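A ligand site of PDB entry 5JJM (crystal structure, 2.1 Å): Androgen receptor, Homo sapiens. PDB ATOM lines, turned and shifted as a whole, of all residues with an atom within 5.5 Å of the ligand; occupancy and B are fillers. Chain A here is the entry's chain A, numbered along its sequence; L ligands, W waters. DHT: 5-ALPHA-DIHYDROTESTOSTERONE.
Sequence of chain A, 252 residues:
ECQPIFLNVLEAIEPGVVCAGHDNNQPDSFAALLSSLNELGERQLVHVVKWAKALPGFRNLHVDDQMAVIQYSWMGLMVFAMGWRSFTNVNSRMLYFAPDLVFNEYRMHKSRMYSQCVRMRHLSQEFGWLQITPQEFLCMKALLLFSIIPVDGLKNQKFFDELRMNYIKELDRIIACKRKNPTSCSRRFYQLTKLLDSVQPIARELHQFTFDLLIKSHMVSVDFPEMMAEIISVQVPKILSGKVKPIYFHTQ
NH2 of Arg 85 lies within hydrogen-bond range of O of Phe 97 (2.8 Å). SD of Met 78 lies close to OE1 of Gln 44 (3.7 Å). The side-chain amide nitrogen (NE2) of Gln 44 lies close to the guanidinium group (NH2) of Arg 85, 3.3 Å away. O of Leu 34 sits close to ND2 of Asn 38.
The guanidinium group of Arg 85 sits at hydrogen-bond distance from an oxygen (O3) of the ligand (3.0 Å). An oxygen (O17) of the ligand is in hydrogen-bond range of the side-chain hydroxyl (OG1) of Thr 210, at 2.7 Å. The side-chain amide oxygen (OD1) of Asn 38 lies within hydrogen-bond range of an oxygen (O17) of the ligand.
Leu 34 touches the ligand. O of Leu 37 touches C11 of the ligand, at 3.5 Å. CD2 of Leu 40 touches C2 of the ligand, 3.9 Å away. Gln 44 touches the ligand (OE1 to C2, 3.3 Å). Met 75 touches the ligand (CE to C18, 3.6 Å). SD of Met 78 touches C19 of the ligand, at 3.7 Å. Val 79 touches the ligand (CG2 to C6, 3.9 Å). CB of Met 82 touches O3 of the ligand, 3.6 Å away. CD1 of Phe 97 touches O3 of the ligand, at 3.7 Å. Met 113 touches the ligand (CE to C15, 3.98 Å). Phe 224 touches the ligand. CE of Met 228 touches C12 of the ligand, at 3.9 Å. Hydrophobic or aromatic side chains within 4 Å of the ligand: Leu 34, Leu 40, Met 75, Met 78, Val 79, Met 82, Phe 97, Met 113, Phe 224 and Met 228. The nearest printed residue that does not touch the ligand is Gly 41 (4.01 Å).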
ATOM      1  N   LEU A  34     -17.105  37.691  -2.244  1.00  0.00           N
ATOM      2  CA  LEU A  34     -17.490  36.297  -1.839  1.00  0.00           C
ATOM      3  C   LEU A  34     -18.426  35.537  -2.799  1.00  0.00           C
ATOM      4  O   LEU A  34     -18.216  34.386  -3.067  1.00  0.00           O
ATOM      5  CB  LEU A  34     -17.952  36.219  -0.324  1.00  0.00           C
ATOM      6  CG  LEU A  34     -16.805  35.966   0.699  1.00  0.00           C
ATOM      7  CD1 LEU A  34     -16.129  34.629   0.363  1.00  0.00           C
ATOM      8  CD2 LEU A  34     -15.728  37.068   0.631  1.00  0.00           C
ATOM      9  N   LEU A  37     -16.104  34.372  -5.350  1.00  0.00           N
ATOM     10  CA  LEU A  37     -15.239  33.283  -4.972  1.00  0.00           C
ATOM     11  C   LEU A  37     -16.089  31.923  -4.987  1.00  0.00           C
ATOM     12  O   LEU A  37     -15.661  30.906  -5.526  1.00  0.00           O
ATOM     13  CB  LEU A  37     -14.630  33.524  -3.598  1.00  0.00           C
ATOM     14  CG  LEU A  37     -13.426  34.419  -3.511  1.00  0.00           C
ATOM     15  CD1 LEU A  37     -13.095  34.709  -2.044  1.00  0.00           C
ATOM     16  CD2 LEU A  37     -12.291  33.693  -4.300  1.00  0.00           C
ATOM     17  N   ASN A  38     -17.323  31.987  -4.472  1.00  0.00           N
ATOM     18  CA  ASN A  38     -18.233  30.818  -4.409  1.00  0.00           C
ATOM     19  C   ASN A  38     -18.545  30.380  -5.846  1.00  0.00           C
ATOM     20  O   ASN A  38     -18.505  29.189  -6.085  1.00  0.00           O
ATOM     21  CB  ASN A  38     -19.589  31.152  -3.726  1.00  0.00           C
ATOM     22  CG  ASN A  38     -19.430  31.408  -2.292  1.00  0.00           C
ATOM     23  OD1 ASN A  38     -18.469  30.955  -1.729  1.00  0.00           O
ATOM     24  ND2 ASN A  38     -20.366  32.166  -1.644  1.00  0.00           N
ATOM     25  N   LEU A  40     -16.589  30.915  -8.431  1.00  0.00           N
ATOM     26  CA  LEU A  40     -15.329  30.324  -8.940  1.00  0.00           C
ATOM     27  C   LEU A  40     -15.194  28.908  -8.393  1.00  0.00           C
ATOM     28  O   LEU A  40     -14.708  28.005  -9.120  1.00  0.00           O
ATOM     29  CB  LEU A  40     -14.092  31.137  -8.492  1.00  0.00           C
ATOM     30  CG  LEU A  40     -12.713  30.523  -8.877  1.00  0.00           C
ATOM     31  CD1 LEU A  40     -12.502  30.238 -10.377  1.00  0.00           C
ATOM     32  CD2 LEU A  40     -11.560  31.377  -8.347  1.00  0.00           C
ATOM     33  N   GLY A  41     -15.506  28.748  -7.103  1.00  0.00           N
ATOM     34  CA  GLY A  41     -15.494  27.362  -6.491  1.00  0.00           C
ATOM     35  C   GLY A  41     -16.359  26.309  -7.218  1.00  0.00           C
ATOM     36  O   GLY A  41     -15.920  25.157  -7.472  1.00  0.00           O
ATOM     37  N   GLN A  44     -14.694  25.465 -10.523  1.00  0.00           N
ATOM     38  CA  GLN A  44     -13.512  24.601 -10.224  1.00  0.00           C
ATOM     39  C   GLN A  44     -13.809  23.222  -9.835  1.00  0.00           C
ATOM     40  O   GLN A  44     -13.110  22.283 -10.208  1.00  0.00           O
ATOM     41  CB  GLN A  44     -12.591  25.238  -9.230  1.00  0.00           C
ATOM     42  CG  GLN A  44     -11.801  26.383  -9.922  1.00  0.00           C
ATOM     43  CD  GLN A  44     -10.627  26.879  -9.132  1.00  0.00           C
ATOM     44  OE1 GLN A  44     -10.261  26.274  -8.108  1.00  0.00           O
ATOM     45  NE2 GLN A  44      -9.998  27.970  -9.569  1.00  0.00           N
ATOM     46  N   TRP A  74     -11.610  18.918  -1.692  1.00  0.00           N
ATOM     47  CA  TRP A  74     -11.663  19.985  -2.685  1.00  0.00           C
ATOM     48  C   TRP A  74     -11.017  21.330  -2.193  1.00  0.00           C
ATOM     49  O   TRP A  74     -10.256  21.919  -2.915  1.00  0.00           O
ATOM     50  CB  TRP A  74     -13.040  20.183  -3.269  1.00  0.00           C
ATOM     51  CG  TRP A  74     -14.035  20.663  -2.333  1.00  0.00           C
ATOM     52  CD1 TRP A  74     -14.910  19.871  -1.626  1.00  0.00           C
ATOM     53  CD2 TRP A  74     -14.299  22.035  -1.943  1.00  0.00           C
ATOM     54  NE1 TRP A  74     -15.682  20.664  -0.797  1.00  0.00           N
ATOM     55  CE2 TRP A  74     -15.373  21.989  -0.977  1.00  0.00           C
ATOM     56  CE3 TRP A  74     -13.744  23.319  -2.333  1.00  0.00           C
ATOM     57  CZ2 TRP A  74     -15.897  23.159  -0.323  1.00  0.00           C
ATOM     58  CZ3 TRP A  74     -14.273  24.488  -1.746  1.00  0.00           C
ATOM     59  CH2 TRP A  74     -15.376  24.386  -0.723  1.00  0.00           C
ATOM     60  N   MET A  75     -11.217  21.692  -0.929  1.00  0.00           N
ATOM     61  CA  MET A  75     -10.695  22.924  -0.390  1.00  0.00           C
ATOM     62  C   MET A  75      -9.147  22.961  -0.474  1.00  0.00           C
ATOM     63  O   MET A  75      -8.587  23.881  -1.086  1.00  0.00           O
ATOM     64  CB  MET A  75     -11.160  23.194   1.062  1.00  0.00           C
ATOM     65  CG  MET A  75     -10.702  24.596   1.566  1.00  0.00           C
ATOM     66  SD  MET A  75     -11.698  25.926   0.882  1.00  0.00           S
ATOM     67  CE  MET A  75     -13.216  25.863   1.858  1.00  0.00           C
ATOM     68  N   MET A  78      -8.009  23.050  -4.266  1.00  0.00           N
ATOM     69  CA  MET A  78      -8.122  24.347  -4.932  1.00  0.00           C
ATOM     70  C   MET A  78      -7.217  25.410  -4.277  1.00  0.00           C
ATOM     71  O   MET A  78      -6.710  26.199  -5.034  1.00  0.00           O
ATOM     72  CB  MET A  78      -9.518  24.874  -5.042  1.00  0.00           C
ATOM     73  CG  MET A  78     -10.443  23.849  -5.755  1.00  0.00           C
ATOM     74  SD  MET A  78     -12.108  24.453  -5.423  1.00  0.00           S
ATOM     75  CE  MET A  78     -12.963  23.099  -6.212  1.00  0.00           C
ATOM     76  N   VAL A  79      -6.938  25.321  -2.959  1.00  0.00           N
ATOM     77  CA  VAL A  79      -5.985  26.241  -2.280  1.00  0.00           C
ATOM     78  C   VAL A  79      -4.584  26.060  -2.786  1.00  0.00           C
ATOM     79  O   VAL A  79      -3.939  27.027  -3.134  1.00  0.00           O
ATOM     80  CB  VAL A  79      -6.032  26.174  -0.734  1.00  0.00           C
ATOM     81  CG1 VAL A  79      -4.917  26.973  -0.037  1.00  0.00           C
ATOM     82  CG2 VAL A  79      -7.279  26.912  -0.361  1.00  0.00           C
ATOM     83  N   MET A  82      -4.177  27.363  -6.523  1.00  0.00           N
ATOM     84  CA  MET A  82      -4.239  28.847  -6.563  1.00  0.00           C
ATOM     85  C   MET A  82      -2.835  29.401  -6.162  1.00  0.00           C
ATOM     86  O   MET A  82      -2.394  30.420  -6.697  1.00  0.00           O
ATOM     87  CB  MET A  82      -5.324  29.336  -5.552  1.00  0.00           C
ATOM     88  CG  MET A  82      -5.622  30.878  -5.659  1.00  0.00           C
ATOM     89  SD  MET A  82      -4.571  31.683  -4.416  1.00  0.00           S
ATOM     90  CE  MET A  82      -5.378  30.949  -2.881  1.00  0.00           C
ATOM     91  N   ARG A  85      -0.602  29.035  -9.107  1.00  0.00           N
ATOM     92  CA  ARG A  85      -0.992  29.997 -10.103  1.00  0.00           C
ATOM     93  C   ARG A  85      -0.588  31.412  -9.675  1.00  0.00           C
ATOM     94  O   ARG A  85      -0.357  32.309 -10.511  1.00  0.00           O
ATOM     95  CB  ARG A  85      -2.515  30.123 -10.202  1.00  0.00           C
ATOM     96  CG  ARG A  85      -3.178  29.045 -10.957  1.00  0.00           C
ATOM     97  CD  ARG A  85      -4.568  29.580 -11.351  1.00  0.00           C
ATOM     98  NE  ARG A  85      -5.456  29.888 -10.242  1.00  0.00           N
ATOM     99  CZ  ARG A  85      -6.170  28.932  -9.565  1.00  0.00           C
ATOM    100  NH1 ARG A  85      -5.996  27.633  -9.824  1.00  0.00           N
ATOM    101  NH2 ARG A  85      -7.070  29.259  -8.619  1.00  0.00           N
ATOM    102  N   PHE A  97      -6.765  34.057  -7.831  1.00  0.00           N
ATOM    103  CA  PHE A  97      -7.902  33.129  -7.805  1.00  0.00           C
ATOM    104  C   PHE A  97      -8.315  32.744  -9.202  1.00  0.00           C
ATOM    105  O   PHE A  97      -8.469  31.512  -9.453  1.00  0.00           O
ATOM    106  CB  PHE A  97      -9.100  33.727  -7.038  1.00  0.00           C
ATOM    107  CG  PHE A  97      -8.829  33.880  -5.547  1.00  0.00           C
ATOM    108  CD1 PHE A  97      -8.733  32.740  -4.728  1.00  0.00           C
ATOM    109  CD2 PHE A  97      -8.683  35.143  -4.958  1.00  0.00           C
ATOM    110  CE1 PHE A  97      -8.530  32.847  -3.312  1.00  0.00           C
ATOM    111  CE2 PHE A  97      -8.467  35.265  -3.553  1.00  0.00           C
ATOM    112  CZ  PHE A  97      -8.429  34.145  -2.746  1.00  0.00           C
ATOM    113  N   MET A 113     -11.447  38.004   5.228  1.00  0.00           N
ATOM    114  CA  MET A 113     -10.542  36.906   5.576  1.00  0.00           C
ATOM    115  C   MET A 113      -9.103  37.173   5.331  1.00  0.00           C
ATOM    116  O   MET A 113      -8.390  36.352   4.718  1.00  0.00           O
ATOM    117  CB  MET A 113     -10.950  35.589   4.927  1.00  0.00           C
ATOM    118  CG  MET A 113     -11.250  35.707   3.458  1.00  0.00           C
ATOM    119  SD  MET A 113     -12.049  34.130   2.978  1.00  0.00           S
ATOM    120  CE  MET A 113     -11.270  34.258   1.339  1.00  0.00           C
ATOM    121  N   MET A 120      -2.469  31.871   2.844  1.00  0.00           N
ATOM    122  CA  MET A 120      -2.338  31.471   1.404  1.00  0.00           C
ATOM    123  C   MET A 120      -1.140  32.128   0.641  1.00  0.00           C
ATOM    124  O   MET A 120      -0.386  31.446  -0.095  1.00  0.00           O
ATOM    125  CB  MET A 120      -3.690  31.734   0.753  1.00  0.00           C
ATOM    126  CG  MET A 120      -4.756  30.812   1.408  1.00  0.00           C
ATOM    127  SD  MET A 120      -6.302  30.779   0.522  1.00  0.00           S
ATOM    128  CE  MET A 120      -7.058  32.286   1.118  1.00  0.00           C
ATOM    129  N   LEU A 206     -10.539  27.743   6.378  1.00  0.00           N
ATOM    130  CA  LEU A 206     -11.503  28.135   5.292  1.00  0.00           C
ATOM    131  C   LEU A 206     -12.836  27.315   5.427  1.00  0.00           C
ATOM    132  O   LEU A 206     -13.903  27.779   5.071  1.00  0.00           O
ATOM    133  CB  LEU A 206     -10.877  27.942   3.875  1.00  0.00           C
ATOM    134  CG  LEU A 206      -9.612  28.815   3.672  1.00  0.00           C
ATOM    135  CD1 LEU A 206      -8.880  28.484   2.381  1.00  0.00           C
ATOM    136  CD2 LEU A 206     -10.013  30.315   3.610  1.00  0.00           C
ATOM    137  N   PHE A 209     -14.793  29.059   8.210  1.00  0.00           N
ATOM    138  CA  PHE A 209     -15.258  30.339   7.611  1.00  0.00           C
ATOM    139  C   PHE A 209     -16.422  30.100   6.607  1.00  0.00           C
ATOM    140  O   PHE A 209     -17.395  30.776   6.675  1.00  0.00           O
ATOM    141  CB  PHE A 209     -14.047  31.073   6.968  1.00  0.00           C
ATOM    142  CG  PHE A 209     -14.385  32.467   6.514  1.00  0.00           C
ATOM    143  CD1 PHE A 209     -14.952  32.683   5.244  1.00  0.00           C
ATOM    144  CD2 PHE A 209     -14.198  33.578   7.410  1.00  0.00           C
ATOM    145  CE1 PHE A 209     -15.281  33.988   4.816  1.00  0.00           C
ATOM    146  CE2 PHE A 209     -14.546  34.853   6.981  1.00  0.00           C
ATOM    147  CZ  PHE A 209     -15.070  35.052   5.655  1.00  0.00           C
ATOM    148  N   THR A 210     -16.344  29.154   5.673  1.00  0.00           N
ATOM    149  CA  THR A 210     -17.368  29.149   4.627  1.00  0.00           C
ATOM    150  C   THR A 210     -18.691  28.533   5.245  1.00  0.00           C
ATOM    151  O   THR A 210     -19.804  28.749   4.717  1.00  0.00           O
ATOM    152  CB  THR A 210     -16.915  28.284   3.404  1.00  0.00           C
ATOM    153  OG1 THR A 210     -17.796  28.456   2.302  1.00  0.00           O
ATOM    154  CG2 THR A 210     -16.863  26.736   3.661  1.00  0.00           C
ATOM    155  N   LEU A 213     -20.297  31.367   7.129  1.00  0.00           N
ATOM    156  CA  LEU A 213     -20.899  32.222   6.080  1.00  0.00           C
ATOM    157  C   LEU A 213     -22.089  31.653   5.308  1.00  0.00           C
ATOM    158  O   LEU A 213     -23.074  32.357   4.952  1.00  0.00           O
ATOM    159  CB  LEU A 213     -19.803  32.715   5.100  1.00  0.00           C
ATOM    160  CG  LEU A 213     -20.203  33.562   3.891  1.00  0.00           C
ATOM    161  CD1 LEU A 213     -20.829  34.857   4.416  1.00  0.00           C
ATOM    162  CD2 LEU A 213     -18.987  33.752   3.005  1.00  0.00           C
ATOM    163  N   PHE A 224     -24.415  31.556  -2.678  1.00  0.00           N
ATOM    164  CA  PHE A 224     -23.753  30.235  -2.813  1.00  0.00           C
ATOM    165  C   PHE A 224     -24.438  29.402  -3.908  1.00  0.00           C
ATOM    166  O   PHE A 224     -25.604  29.086  -3.735  1.00  0.00           O
ATOM    167  CB  PHE A 224     -23.836  29.408  -1.550  1.00  0.00           C
ATOM    168  CG  PHE A 224     -22.859  29.782  -0.534  1.00  0.00           C
ATOM    169  CD1 PHE A 224     -23.062  30.930   0.268  1.00  0.00           C
ATOM    170  CD2 PHE A 224     -21.725  29.032  -0.361  1.00  0.00           C
ATOM    171  CE1 PHE A 224     -22.100  31.312   1.229  1.00  0.00           C
ATOM    172  CE2 PHE A 224     -20.763  29.398   0.567  1.00  0.00           C
ATOM    173  CZ  PHE A 224     -20.968  30.550   1.382  1.00  0.00           C
ATOM    174  N   MET A 228     -22.034  23.735  -4.375  1.00  0.00           N
ATOM    175  CA  MET A 228     -21.268  24.239  -3.236  1.00  0.00           C
ATOM    176  C   MET A 228     -22.072  24.269  -1.904  1.00  0.00           C
ATOM    177  O   MET A 228     -21.605  23.835  -0.850  1.00  0.00           O
ATOM    178  CB  MET A 228     -20.752  25.626  -3.601  1.00  0.00           C
ATOM    179  CG  MET A 228     -19.602  25.569  -4.595  1.00  0.00           C
ATOM    180  SD  MET A 228     -17.921  25.349  -3.924  1.00  0.00           S
ATOM    181  CE  MET A 228     -17.931  26.796  -2.836  1.00  0.00           C
ATOM    182  N   ILE A 232     -21.093  21.947   1.335  1.00  0.00           N
ATOM    183  CA  ILE A 232     -20.726  22.668   2.587  1.00  0.00           C
ATOM    184  C   ILE A 232     -21.730  22.466   3.761  1.00  0.00           C
ATOM    185  O   ILE A 232     -21.319  22.307   4.937  1.00  0.00           O
ATOM    186  CB  ILE A 232     -20.497  24.174   2.368  1.00  0.00           C
ATOM    187  CG1 ILE A 232     -19.269  24.415   1.387  1.00  0.00           C
ATOM    188  CG2 ILE A 232     -20.173  24.910   3.714  1.00  0.00           C
ATOM    189  CD1 ILE A 232     -19.300  25.773   0.699  1.00  0.00           C
HETATM  190  C1  DHT L   1     -12.206  28.985  -4.845  1.00  0.00           C
HETATM  191  C2  DHT L   1     -11.103  28.463  -5.822  1.00  0.00           C
HETATM  192  C3  DHT L   1      -9.734  28.913  -5.365  1.00  0.00           C
HETATM  193  O3  DHT L   1      -8.884  29.301  -6.204  1.00  0.00           O
HETATM  194  C4  DHT L   1      -9.344  28.850  -3.916  1.00  0.00           C
HETATM  195  C5  DHT L   1     -10.433  29.470  -3.099  1.00  0.00           C
HETATM  196  C6  DHT L   1      -9.978  29.463  -1.621  1.00  0.00           C
HETATM  197  C7  DHT L   1     -11.051  30.070  -0.723  1.00  0.00           C
HETATM  198  C8  DHT L   1     -12.464  29.524  -1.076  1.00  0.00           C
HETATM  199  C9  DHT L   1     -12.876  29.595  -2.560  1.00  0.00           C
HETATM  200  C10 DHT L   1     -11.791  28.839  -3.369  1.00  0.00           C
HETATM  201  C11 DHT L   1     -14.303  29.053  -2.857  1.00  0.00           C
HETATM  202  C12 DHT L   1     -15.430  29.707  -2.046  1.00  0.00           C
HETATM  203  C13 DHT L   1     -14.987  29.796  -0.567  1.00  0.00           C
HETATM  204  C14 DHT L   1     -13.537  30.366  -0.446  1.00  0.00           C
HETATM  205  C15 DHT L   1     -13.321  30.862   0.985  1.00  0.00           C
HETATM  206  C16 DHT L   1     -14.781  31.186   1.384  1.00  0.00           C
HETATM  207  C17 DHT L   1     -15.777  30.848   0.222  1.00  0.00           C
HETATM  208  O17 DHT L   1     -17.220  30.556   0.629  1.00  0.00           O
HETATM  209  C18 DHT L   1     -15.168  28.380   0.090  1.00  0.00           C
HETATM  210  C19 DHT L   1     -11.725  27.304  -3.048  1.00  0.00           C
HETATM  211  O   HOH W   1      -7.638  26.645  -7.338  1.00  0.00           O
